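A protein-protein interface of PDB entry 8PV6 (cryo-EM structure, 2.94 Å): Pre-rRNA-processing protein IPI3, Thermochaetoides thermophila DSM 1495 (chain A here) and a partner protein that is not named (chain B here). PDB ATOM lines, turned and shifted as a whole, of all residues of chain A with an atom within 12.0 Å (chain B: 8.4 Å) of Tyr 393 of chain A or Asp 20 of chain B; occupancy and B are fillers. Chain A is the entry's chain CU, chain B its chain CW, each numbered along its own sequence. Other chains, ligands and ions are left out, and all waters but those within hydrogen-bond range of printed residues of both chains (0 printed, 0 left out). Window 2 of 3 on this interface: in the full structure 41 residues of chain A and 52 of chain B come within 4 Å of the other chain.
The side-chain hydroxyl (OG) of Ser 118 of chain B lies within hydrogen-bond range of the backbone carbonyl oxygen (O) of Ala 388 of chain A (3.3 Å). The side-chain hydroxyl (OH) of Tyr 393 of chain A lies within hydrogen-bond range of the backbone carbonyl oxygen (O) of Asp 20 of chain B (2.7 Å).
OG1 of Thr 80 of chain B lies within hydrogen-bond range of O of Ala 76 of chain B, at 2.8 Å.
Pro 23 of chain B touches Ile 389 of chain A. CG1 of Ile 389 of chain A touches CE2 of Phe 79 of chain B, at 3.8 Å. Ala 391 of chain A touches Ser 118 of chain B (CB to OG, 3.2 Å). CZ of Phe 392 of chain A touches C of Pro 75 of chain B, 3.97 Å away. CZ of Phe 392 of chain A touches CA of Ala 76 of chain B, at 3.6 Å. Pro 116 of chain B touches Phe 392 of chain A (CG to CE1, 3.6 Å). Phe 392 of chain A touches Ser 118 of chain B (N to OG, 3.8 Å). CB of Pro 23 of chain B touches OH of Tyr 393 of chain A (3.5 Å). Tyr 393 of chain A touches Arg 24 of chain B.
Of chain B, only Asp 20 (2.7 Å), Pro 23 (3.5 Å) and Arg 24 (3.6 Å) come within 4 Å of Tyr 393 of chain A. Printed residues of chain A within 4 Å of Asp 20 of chain B: Tyr 393 (2.7 Å). No residue of chain A comes within 4 Å of Pro 18 of chain B. No residue of chain A comes within 4 Å of Val 19 of chain B. No residue of chain A comes within 4 Å of Ser 21 of chain B. No residue of chain A comes within 4 Å of Leu 22 of chain B. No residue of chain A comes within 4 Å of Ser 74 of chain B. Ala 76 of chain B touches one residue of chain A. Of the printed residues of chain A, Phe 79 of chain B touches Ile 389. Of the printed residues of chain B, Ile 389 of chain A touches Pro 23 (3.3 Å) and Phe 79 (3.8 Å). Printed residues of chain B within 4 Å of Ala 391 of chain A: Ser 118. Printed residues of chain B within 4 Å of Ala 388 of chain A: Ser 118 (3.3 Å). Of the printed residues of chain A, Pro 75 of chain B touches Phe 392 (3.97 Å). Ala 384 of chain A touches none of the printed residues of chain B. The nearest residue of chain B that does not touch Tyr 393 of chain A is Ser 21 of chain B (4.3 Å).
Printed residues of chain B that touch a printed residue of chain A: Asp 20, Pro 23, Arg 24, Pro 75, Ala 76, Phe 79, Pro 116 and Ser 118. Hydrophobic or aromatic side chains of chain B that line the printed part of chain A: Pro 23, Phe 79 and Pro 116. Printed residues of chain A that touch a printed residue of chain B: Ala 388, Ile 389, Ala 391, Phe 392 and Tyr 393. Among the printed residues, 11 pairs touch across the chains. Among the printed residues, no Asp or Glu carboxylate lies within 4 Å of a Lys or Arg side-chain nitrogen of the other chain.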
ATOM      1  N   ALA A 384      -5.002  25.347 -21.297  1.00  0.00           N
ATOM      2  CA  ALA A 384      -4.979  24.760 -22.630  1.00  0.00           C
ATOM      3  C   ALA A 384      -3.579  24.809 -23.231  1.00  0.00           C
ATOM      4  O   ALA A 384      -3.178  23.885 -23.948  1.00  0.00           O
ATOM      5  CB  ALA A 384      -5.980  25.476 -23.537  1.00  0.00           C
ATOM      6  N   LEU A 385      -2.806  25.859 -22.930  1.00  0.00           N
ATOM      7  CA  LEU A 385      -1.467  25.950 -23.509  1.00  0.00           C
ATOM      8  C   LEU A 385      -0.508  24.937 -22.892  1.00  0.00           C
ATOM      9  O   LEU A 385       0.248  24.282 -23.620  1.00  0.00           O
ATOM     10  CB  LEU A 385      -0.922  27.371 -23.386  1.00  0.00           C
ATOM     11  CG  LEU A 385       0.331  27.630 -24.221  1.00  0.00           C
ATOM     12  CD1 LEU A 385      -0.040  27.785 -25.676  1.00  0.00           C
ATOM     13  CD2 LEU A 385       1.036  28.875 -23.728  1.00  0.00           C
ATOM     14  N   GLU A 386      -0.516  24.782 -21.557  1.00  0.00           N
ATOM     15  CA  GLU A 386       0.321  23.712 -20.993  1.00  0.00           C
ATOM     16  C   GLU A 386      -0.175  22.328 -21.402  1.00  0.00           C
ATOM     17  O   GLU A 386       0.637  21.411 -21.563  1.00  0.00           O
ATOM     18  CB  GLU A 386       0.515  23.731 -19.463  1.00  0.00           C
ATOM     19  CG  GLU A 386       1.335  24.863 -18.804  1.00  0.00           C
ATOM     20  CD  GLU A 386       0.604  26.136 -18.504  1.00  0.00           C
ATOM     21  OE1 GLU A 386      -0.610  26.181 -18.726  1.00  0.00           O
ATOM     22  OE2 GLU A 386       1.252  27.098 -18.037  1.00  0.00           O
ATOM     23  N   SER A 387      -1.491  22.154 -21.585  1.00  0.00           N
ATOM     24  CA  SER A 387      -1.988  20.872 -22.078  1.00  0.00           C
ATOM     25  C   SER A 387      -1.466  20.580 -23.480  1.00  0.00           C
ATOM     26  O   SER A 387      -1.032  19.456 -23.770  1.00  0.00           O
ATOM     27  CB  SER A 387      -3.518  20.858 -22.064  1.00  0.00           C
ATOM     28  OG  SER A 387      -4.027  19.643 -22.592  1.00  0.00           O
ATOM     29  N   ALA A 388      -1.469  21.594 -24.350  1.00  0.00           N
ATOM     30  CA  ALA A 388      -0.961  21.427 -25.706  1.00  0.00           C
ATOM     31  C   ALA A 388       0.536  21.145 -25.711  1.00  0.00           C
ATOM     32  O   ALA A 388       1.005  20.293 -26.471  1.00  0.00           O
ATOM     33  CB  ALA A 388      -1.276  22.666 -26.542  1.00  0.00           C
ATOM     34  N   ILE A 389       1.301  21.839 -24.859  1.00  0.00           N
ATOM     35  CA  ILE A 389       2.747  21.616 -24.801  1.00  0.00           C
ATOM     36  C   ILE A 389       3.061  20.209 -24.302  1.00  0.00           C
ATOM     37  O   ILE A 389       3.919  19.513 -24.864  1.00  0.00           O
ATOM     38  CB  ILE A 389       3.420  22.692 -23.927  1.00  0.00           C
ATOM     39  CG1 ILE A 389       3.280  24.069 -24.571  1.00  0.00           C
ATOM     40  CG2 ILE A 389       4.891  22.383 -23.735  1.00  0.00           C
ATOM     41  CD1 ILE A 389       3.484  25.206 -23.600  1.00  0.00           C
ATOM     42  N   VAL A 390       2.364  19.761 -23.250  1.00  0.00           N
ATOM     43  CA  VAL A 390       2.611  18.430 -22.696  1.00  0.00           C
ATOM     44  C   VAL A 390       2.235  17.348 -23.702  1.00  0.00           C
ATOM     45  O   VAL A 390       2.977  16.375 -23.892  1.00  0.00           O
ATOM     46  CB  VAL A 390       1.861  18.264 -21.360  1.00  0.00           C
ATOM     47  CG1 VAL A 390       1.833  16.809 -20.924  1.00  0.00           C
ATOM     48  CG2 VAL A 390       2.519  19.107 -20.284  1.00  0.00           C
ATOM     49  N   ALA A 391       1.100  17.510 -24.390  1.00  0.00           N
ATOM     50  CA  ALA A 391       0.709  16.517 -25.385  1.00  0.00           C
ATOM     51  C   ALA A 391       1.609  16.576 -26.616  1.00  0.00           C
ATOM     52  O   ALA A 391       1.740  15.587 -27.346  1.00  0.00           O
ATOM     53  CB  ALA A 391      -0.757  16.707 -25.769  1.00  0.00           C
ATOM     54  N   PHE A 392       2.232  17.730 -26.866  1.00  0.00           N
ATOM     55  CA  PHE A 392       3.242  17.819 -27.916  1.00  0.00           C
ATOM     56  C   PHE A 392       4.488  17.028 -27.542  1.00  0.00           C
ATOM     57  O   PHE A 392       5.029  16.280 -28.364  1.00  0.00           O
ATOM     58  CB  PHE A 392       3.584  19.287 -28.178  1.00  0.00           C
ATOM     59  CG  PHE A 392       4.693  19.496 -29.171  1.00  0.00           C
ATOM     60  CD1 PHE A 392       4.438  19.456 -30.530  1.00  0.00           C
ATOM     61  CD2 PHE A 392       5.983  19.767 -28.747  1.00  0.00           C
ATOM     62  CE1 PHE A 392       5.453  19.659 -31.445  1.00  0.00           C
ATOM     63  CE2 PHE A 392       6.998  19.967 -29.657  1.00  0.00           C
ATOM     64  CZ  PHE A 392       6.732  19.912 -31.006  1.00  0.00           C
ATOM     65  N   TYR A 393       4.953  17.176 -26.306  1.00  0.00           N
ATOM     66  CA  TYR A 393       6.145  16.468 -25.852  1.00  0.00           C
ATOM     67  C   TYR A 393       5.808  15.053 -25.394  1.00  0.00           C
ATOM     68  O   TYR A 393       5.257  14.257 -26.154  1.00  0.00           O
ATOM     69  CB  TYR A 393       6.824  17.237 -24.718  1.00  0.00           C
ATOM     70  CG  TYR A 393       7.614  18.437 -25.182  1.00  0.00           C
ATOM     71  CD1 TYR A 393       7.671  19.592 -24.417  1.00  0.00           C
ATOM     72  CD2 TYR A 393       8.310  18.411 -26.382  1.00  0.00           C
ATOM     73  CE1 TYR A 393       8.392  20.691 -24.836  1.00  0.00           C
ATOM     74  CE2 TYR A 393       9.035  19.506 -26.810  1.00  0.00           C
ATOM     75  CZ  TYR A 393       9.071  20.643 -26.033  1.00  0.00           C
ATOM     76  OH  TYR A 393       9.793  21.735 -26.454  1.00  0.00           O
ATOM     77  N   THR B  17      17.194  31.305 -27.876  1.00  0.00           N
ATOM     78  CA  THR B  17      16.630  30.021 -27.481  1.00  0.00           C
ATOM     79  C   THR B  17      16.733  28.996 -28.606  1.00  0.00           C
ATOM     80  O   THR B  17      16.461  29.327 -29.768  1.00  0.00           O
ATOM     81  CB  THR B  17      15.168  30.182 -27.072  1.00  0.00           C
ATOM     82  OG1 THR B  17      15.024  31.333 -26.230  1.00  0.00           O
ATOM     83  CG2 THR B  17      14.687  28.944 -26.340  1.00  0.00           C
ATOM     84  N   PRO B  18      17.134  27.759 -28.312  1.00  0.00           N
ATOM     85  CA  PRO B  18      16.995  26.687 -29.302  1.00  0.00           C
ATOM     86  C   PRO B  18      15.532  26.371 -29.585  1.00  0.00           C
ATOM     87  O   PRO B  18      14.650  26.558 -28.736  1.00  0.00           O
ATOM     88  CB  PRO B  18      17.714  25.496 -28.653  1.00  0.00           C
ATOM     89  CG  PRO B  18      17.993  25.894 -27.243  1.00  0.00           C
ATOM     90  CD  PRO B  18      18.004  27.379 -27.188  1.00  0.00           C
ATOM     91  N   VAL B  19      15.287  25.877 -30.801  1.00  0.00           N
ATOM     92  CA  VAL B  19      13.924  25.604 -31.247  1.00  0.00           C
ATOM     93  C   VAL B  19      13.312  24.462 -30.447  1.00  0.00           C
ATOM     94  O   VAL B  19      12.099  24.435 -30.212  1.00  0.00           O
ATOM     95  CB  VAL B  19      13.901  25.325 -32.762  1.00  0.00           C
ATOM     96  CG1 VAL B  19      14.250  26.585 -33.529  1.00  0.00           C
ATOM     97  CG2 VAL B  19      14.870  24.211 -33.127  1.00  0.00           C
ATOM     98  N   ASP B  20      14.137  23.513 -29.994  1.00  0.00           N
ATOM     99  CA  ASP B  20      13.636  22.382 -29.224  1.00  0.00           C
ATOM    100  C   ASP B  20      13.127  22.784 -27.847  1.00  0.00           C
ATOM    101  O   ASP B  20      12.298  22.066 -27.280  1.00  0.00           O
ATOM    102  CB  ASP B  20      14.726  21.321 -29.083  1.00  0.00           C
ATOM    103  CG  ASP B  20      15.089  20.683 -30.408  1.00  0.00           C
ATOM    104  OD1 ASP B  20      14.347  20.891 -31.390  1.00  0.00           O
ATOM    105  OD2 ASP B  20      16.114  19.972 -30.467  1.00  0.00           O
ATOM    106  N   SER B  21      13.594  23.904 -27.300  1.00  0.00           N
ATOM    107  CA  SER B  21      13.119  24.392 -26.014  1.00  0.00           C
ATOM    108  C   SER B  21      12.238  25.626 -26.140  1.00  0.00           C
ATOM    109  O   SER B  21      11.768  26.137 -25.117  1.00  0.00           O
ATOM    110  CB  SER B  21      14.302  24.699 -25.089  1.00  0.00           C
ATOM    111  OG  SER B  21      15.150  25.676 -25.661  1.00  0.00           O
ATOM    112  N   LEU B  22      12.020  26.130 -27.355  1.00  0.00           N
ATOM    113  CA  LEU B  22      11.061  27.214 -27.571  1.00  0.00           C
ATOM    114  C   LEU B  22       9.617  26.909 -27.135  1.00  0.00           C
ATOM    115  O   LEU B  22       8.972  27.814 -26.586  1.00  0.00           O
ATOM    116  CB  LEU B  22      11.091  27.656 -29.040  1.00  0.00           C
ATOM    117  CG  LEU B  22      12.108  28.738 -29.398  1.00  0.00           C
ATOM    118  CD1 LEU B  22      12.166  28.942 -30.901  1.00  0.00           C
ATOM    119  CD2 LEU B  22      11.762  30.036 -28.695  1.00  0.00           C
ATOM    120  N   PRO B  23       9.042  25.706 -27.373  1.00  0.00           N
ATOM    121  CA  PRO B  23       7.683  25.455 -26.847  1.00  0.00           C
ATOM    122  C   PRO B  23       7.550  25.529 -25.334  1.00  0.00           C
ATOM    123  O   PRO B  23       6.469  25.861 -24.832  1.00  0.00           O
ATOM    124  CB  PRO B  23       7.366  24.052 -27.368  1.00  0.00           C
ATOM    125  CG  PRO B  23       8.102  23.951 -28.597  1.00  0.00           C
ATOM    126  CD  PRO B  23       9.399  24.659 -28.352  1.00  0.00           C
ATOM    127  N   ARG B  24       8.611  25.211 -24.587  1.00  0.00           N
ATOM    128  CA  ARG B  24       8.555  25.356 -23.136  1.00  0.00           C
ATOM    129  C   ARG B  24       8.434  26.817 -22.730  1.00  0.00           C
ATOM    130  O   ARG B  24       7.774  27.134 -21.735  1.00  0.00           O
ATOM    131  CB  ARG B  24       9.788  24.726 -22.491  1.00  0.00           C
ATOM    132  CG  ARG B  24       9.892  23.230 -22.700  1.00  0.00           C
ATOM    133  CD  ARG B  24      10.917  22.610 -21.769  1.00  0.00           C
ATOM    134  NE  ARG B  24      11.219  21.234 -22.142  1.00  0.00           N
ATOM    135  CZ  ARG B  24      12.198  20.879 -22.963  1.00  0.00           C
ATOM    136  NH1 ARG B  24      12.997  21.778 -23.514  1.00  0.00           N
ATOM    137  NH2 ARG B  24      12.379  19.591 -23.238  1.00  0.00           N
ATOM    138  N   LEU B  25       9.051  27.717 -23.489  1.00  0.00           N
ATOM    139  CA  LEU B  25       8.974  29.145 -23.222  1.00  0.00           C
ATOM    140  C   LEU B  25       7.899  29.842 -24.040  1.00  0.00           C
ATOM    141  O   LEU B  25       7.868  31.078 -24.060  1.00  0.00           O
ATOM    142  CB  LEU B  25      10.328  29.810 -23.477  1.00  0.00           C
ATOM    143  CG  LEU B  25      11.594  29.050 -23.087  1.00  0.00           C
ATOM    144  CD1 LEU B  25      12.785  29.914 -23.388  1.00  0.00           C
ATOM    145  CD2 LEU B  25      11.591  28.687 -21.604  1.00  0.00           C
ATOM    146  N   CYS B  26       7.057  29.087 -24.746  1.00  0.00           N
ATOM    147  CA  CYS B  26       5.863  29.675 -25.355  1.00  0.00           C
ATOM    148  C   CYS B  26       4.961  30.450 -24.389  1.00  0.00           C
ATOM    149  O   CYS B  26       4.450  31.502 -24.810  1.00  0.00           O
ATOM    150  CB  CYS B  26       5.053  28.597 -26.089  1.00  0.00           C
ATOM    151  SG  CYS B  26       5.598  28.257 -27.769  1.00  0.00           S
ATOM    152  N   LEU B  69      10.403  30.308 -38.555  1.00  0.00           N
ATOM    153  CA  LEU B  69       9.991  29.178 -37.729  1.00  0.00           C
ATOM    154  C   LEU B  69       8.800  28.455 -38.343  1.00  0.00           C
ATOM    155  O   LEU B  69       8.693  27.226 -38.251  1.00  0.00           O
ATOM    156  CB  LEU B  69       9.660  29.647 -36.312  1.00  0.00           C
ATOM    157  CG  LEU B  69      10.828  30.079 -35.426  1.00  0.00           C
ATOM    158  CD1 LEU B  69      10.319  30.756 -34.166  1.00  0.00           C
ATOM    159  CD2 LEU B  69      11.700  28.887 -35.082  1.00  0.00           C
ATOM    160  N   LYS B  73      12.070  23.433 -40.652  1.00  0.00           N
ATOM    161  CA  LYS B  73      11.915  21.985 -40.556  1.00  0.00           C
ATOM    162  C   LYS B  73      11.519  21.558 -39.148  1.00  0.00           C
ATOM    163  O   LYS B  73      10.992  20.457 -38.955  1.00  0.00           O
ATOM    164  CB  LYS B  73      13.209  21.293 -40.981  1.00  0.00           C
ATOM    165  CG  LYS B  73      13.633  21.594 -42.409  1.00  0.00           C
ATOM    166  CD  LYS B  73      12.644  21.035 -43.416  1.00  0.00           C
ATOM    167  CE  LYS B  73      13.161  21.194 -44.837  1.00  0.00           C
ATOM    168  NZ  LYS B  73      13.193  22.621 -45.261  1.00  0.00           N
ATOM    169  N   SER B  74      11.767  22.406 -38.155  1.00  0.00           N
ATOM    170  CA  SER B  74      11.548  22.017 -36.772  1.00  0.00           C
ATOM    171  C   SER B  74      10.059  22.066 -36.429  1.00  0.00           C
ATOM    172  O   SER B  74       9.443  23.140 -36.516  1.00  0.00           O
ATOM    173  CB  SER B  74      12.332  22.934 -35.833  1.00  0.00           C
ATOM    174  OG  SER B  74      12.231  22.496 -34.489  1.00  0.00           O
ATOM    175  N   PRO B  75       9.452  20.941 -36.035  1.00  0.00           N
ATOM    176  CA  PRO B  75       8.052  20.984 -35.585  1.00  0.00           C
ATOM    177  C   PRO B  75       7.860  21.795 -34.317  1.00  0.00           C
ATOM    178  O   PRO B  75       6.802  22.409 -34.141  1.00  0.00           O
ATOM    179  CB  PRO B  75       7.707  19.506 -35.370  1.00  0.00           C
ATOM    180  CG  PRO B  75       9.016  18.849 -35.123  1.00  0.00           C
ATOM    181  CD  PRO B  75      10.022  19.587 -35.947  1.00  0.00           C
ATOM    182  N   ALA B  76       8.857  21.820 -33.431  1.00  0.00           N
ATOM    183  CA  ALA B  76       8.777  22.660 -32.242  1.00  0.00           C
ATOM    184  C   ALA B  76       8.790  24.140 -32.610  1.00  0.00           C
ATOM    185  O   ALA B  76       8.034  24.938 -32.036  1.00  0.00           O
ATOM    186  CB  ALA B  76       9.925  22.321 -31.298  1.00  0.00           C
ATOM    187  N   GLY B  77       9.632  24.517 -33.574  1.00  0.00           N
ATOM    188  CA  GLY B  77       9.609  25.880 -34.073  1.00  0.00           C
ATOM    189  C   GLY B  77       8.303  26.224 -34.760  1.00  0.00           C
ATOM    190  O   GLY B  77       7.820  27.354 -34.663  1.00  0.00           O
ATOM    191  N   PHE B  79       5.372  24.918 -33.907  1.00  0.00           N
ATOM    192  CA  PHE B  79       4.437  25.097 -32.797  1.00  0.00           C
ATOM    193  C   PHE B  79       4.578  26.485 -32.177  1.00  0.00           C
ATOM    194  O   PHE B  79       3.579  27.174 -31.911  1.00  0.00           O
ATOM    195  CB  PHE B  79       4.690  24.004 -31.755  1.00  0.00           C
ATOM    196  CG  PHE B  79       3.815  24.089 -30.539  1.00  0.00           C
ATOM    197  CD1 PHE B  79       2.545  23.542 -30.550  1.00  0.00           C
ATOM    198  CD2 PHE B  79       4.275  24.680 -29.375  1.00  0.00           C
ATOM    199  CE1 PHE B  79       1.745  23.603 -29.431  1.00  0.00           C
ATOM    200  CE2 PHE B  79       3.474  24.750 -28.255  1.00  0.00           C
ATOM    201  CZ  PHE B  79       2.209  24.211 -28.283  1.00  0.00           C
ATOM    202  N   THR B  80       5.825  26.914 -31.958  1.00  0.00           N
ATOM    203  CA  THR B  80       6.080  28.259 -31.451  1.00  0.00           C
ATOM    204  C   THR B  80       5.579  29.319 -32.424  1.00  0.00           C
ATOM    205  O   THR B  80       5.051  30.357 -32.007  1.00  0.00           O
ATOM    206  CB  THR B  80       7.572  28.443 -31.185  1.00  0.00           C
ATOM    207  OG1 THR B  80       8.082  27.280 -30.527  1.00  0.00           O
ATOM    208  CG2 THR B  80       7.816  29.653 -30.306  1.00  0.00           C
ATOM    209  N   PRO B 116       2.665  17.038 -34.774  1.00  0.00           N
ATOM    210  CA  PRO B 116       1.803  16.578 -33.680  1.00  0.00           C
ATOM    211  C   PRO B 116       0.461  17.298 -33.631  1.00  0.00           C
ATOM    212  O   PRO B 116       0.305  18.451 -34.051  1.00  0.00           O
ATOM    213  CB  PRO B 116       2.636  16.867 -32.429  1.00  0.00           C
ATOM    214  CG  PRO B 116       4.029  16.720 -32.902  1.00  0.00           C
ATOM    215  CD  PRO B 116       4.045  17.265 -34.304  1.00  0.00           C
ATOM    216  N   SER B 118      -1.425  18.438 -31.222  1.00  0.00           N
ATOM    217  CA  SER B 118      -1.584  19.680 -30.472  1.00  0.00           C
ATOM    218  C   SER B 118      -1.241  20.885 -31.336  1.00  0.00           C
ATOM    219  O   SER B 118      -1.967  21.889 -31.334  1.00  0.00           O
ATOM    220  CB  SER B 118      -0.714  19.654 -29.220  1.00  0.00           C
ATOM    221  OG  SER B 118      -1.111  18.603 -28.364  1.00  0.00           O
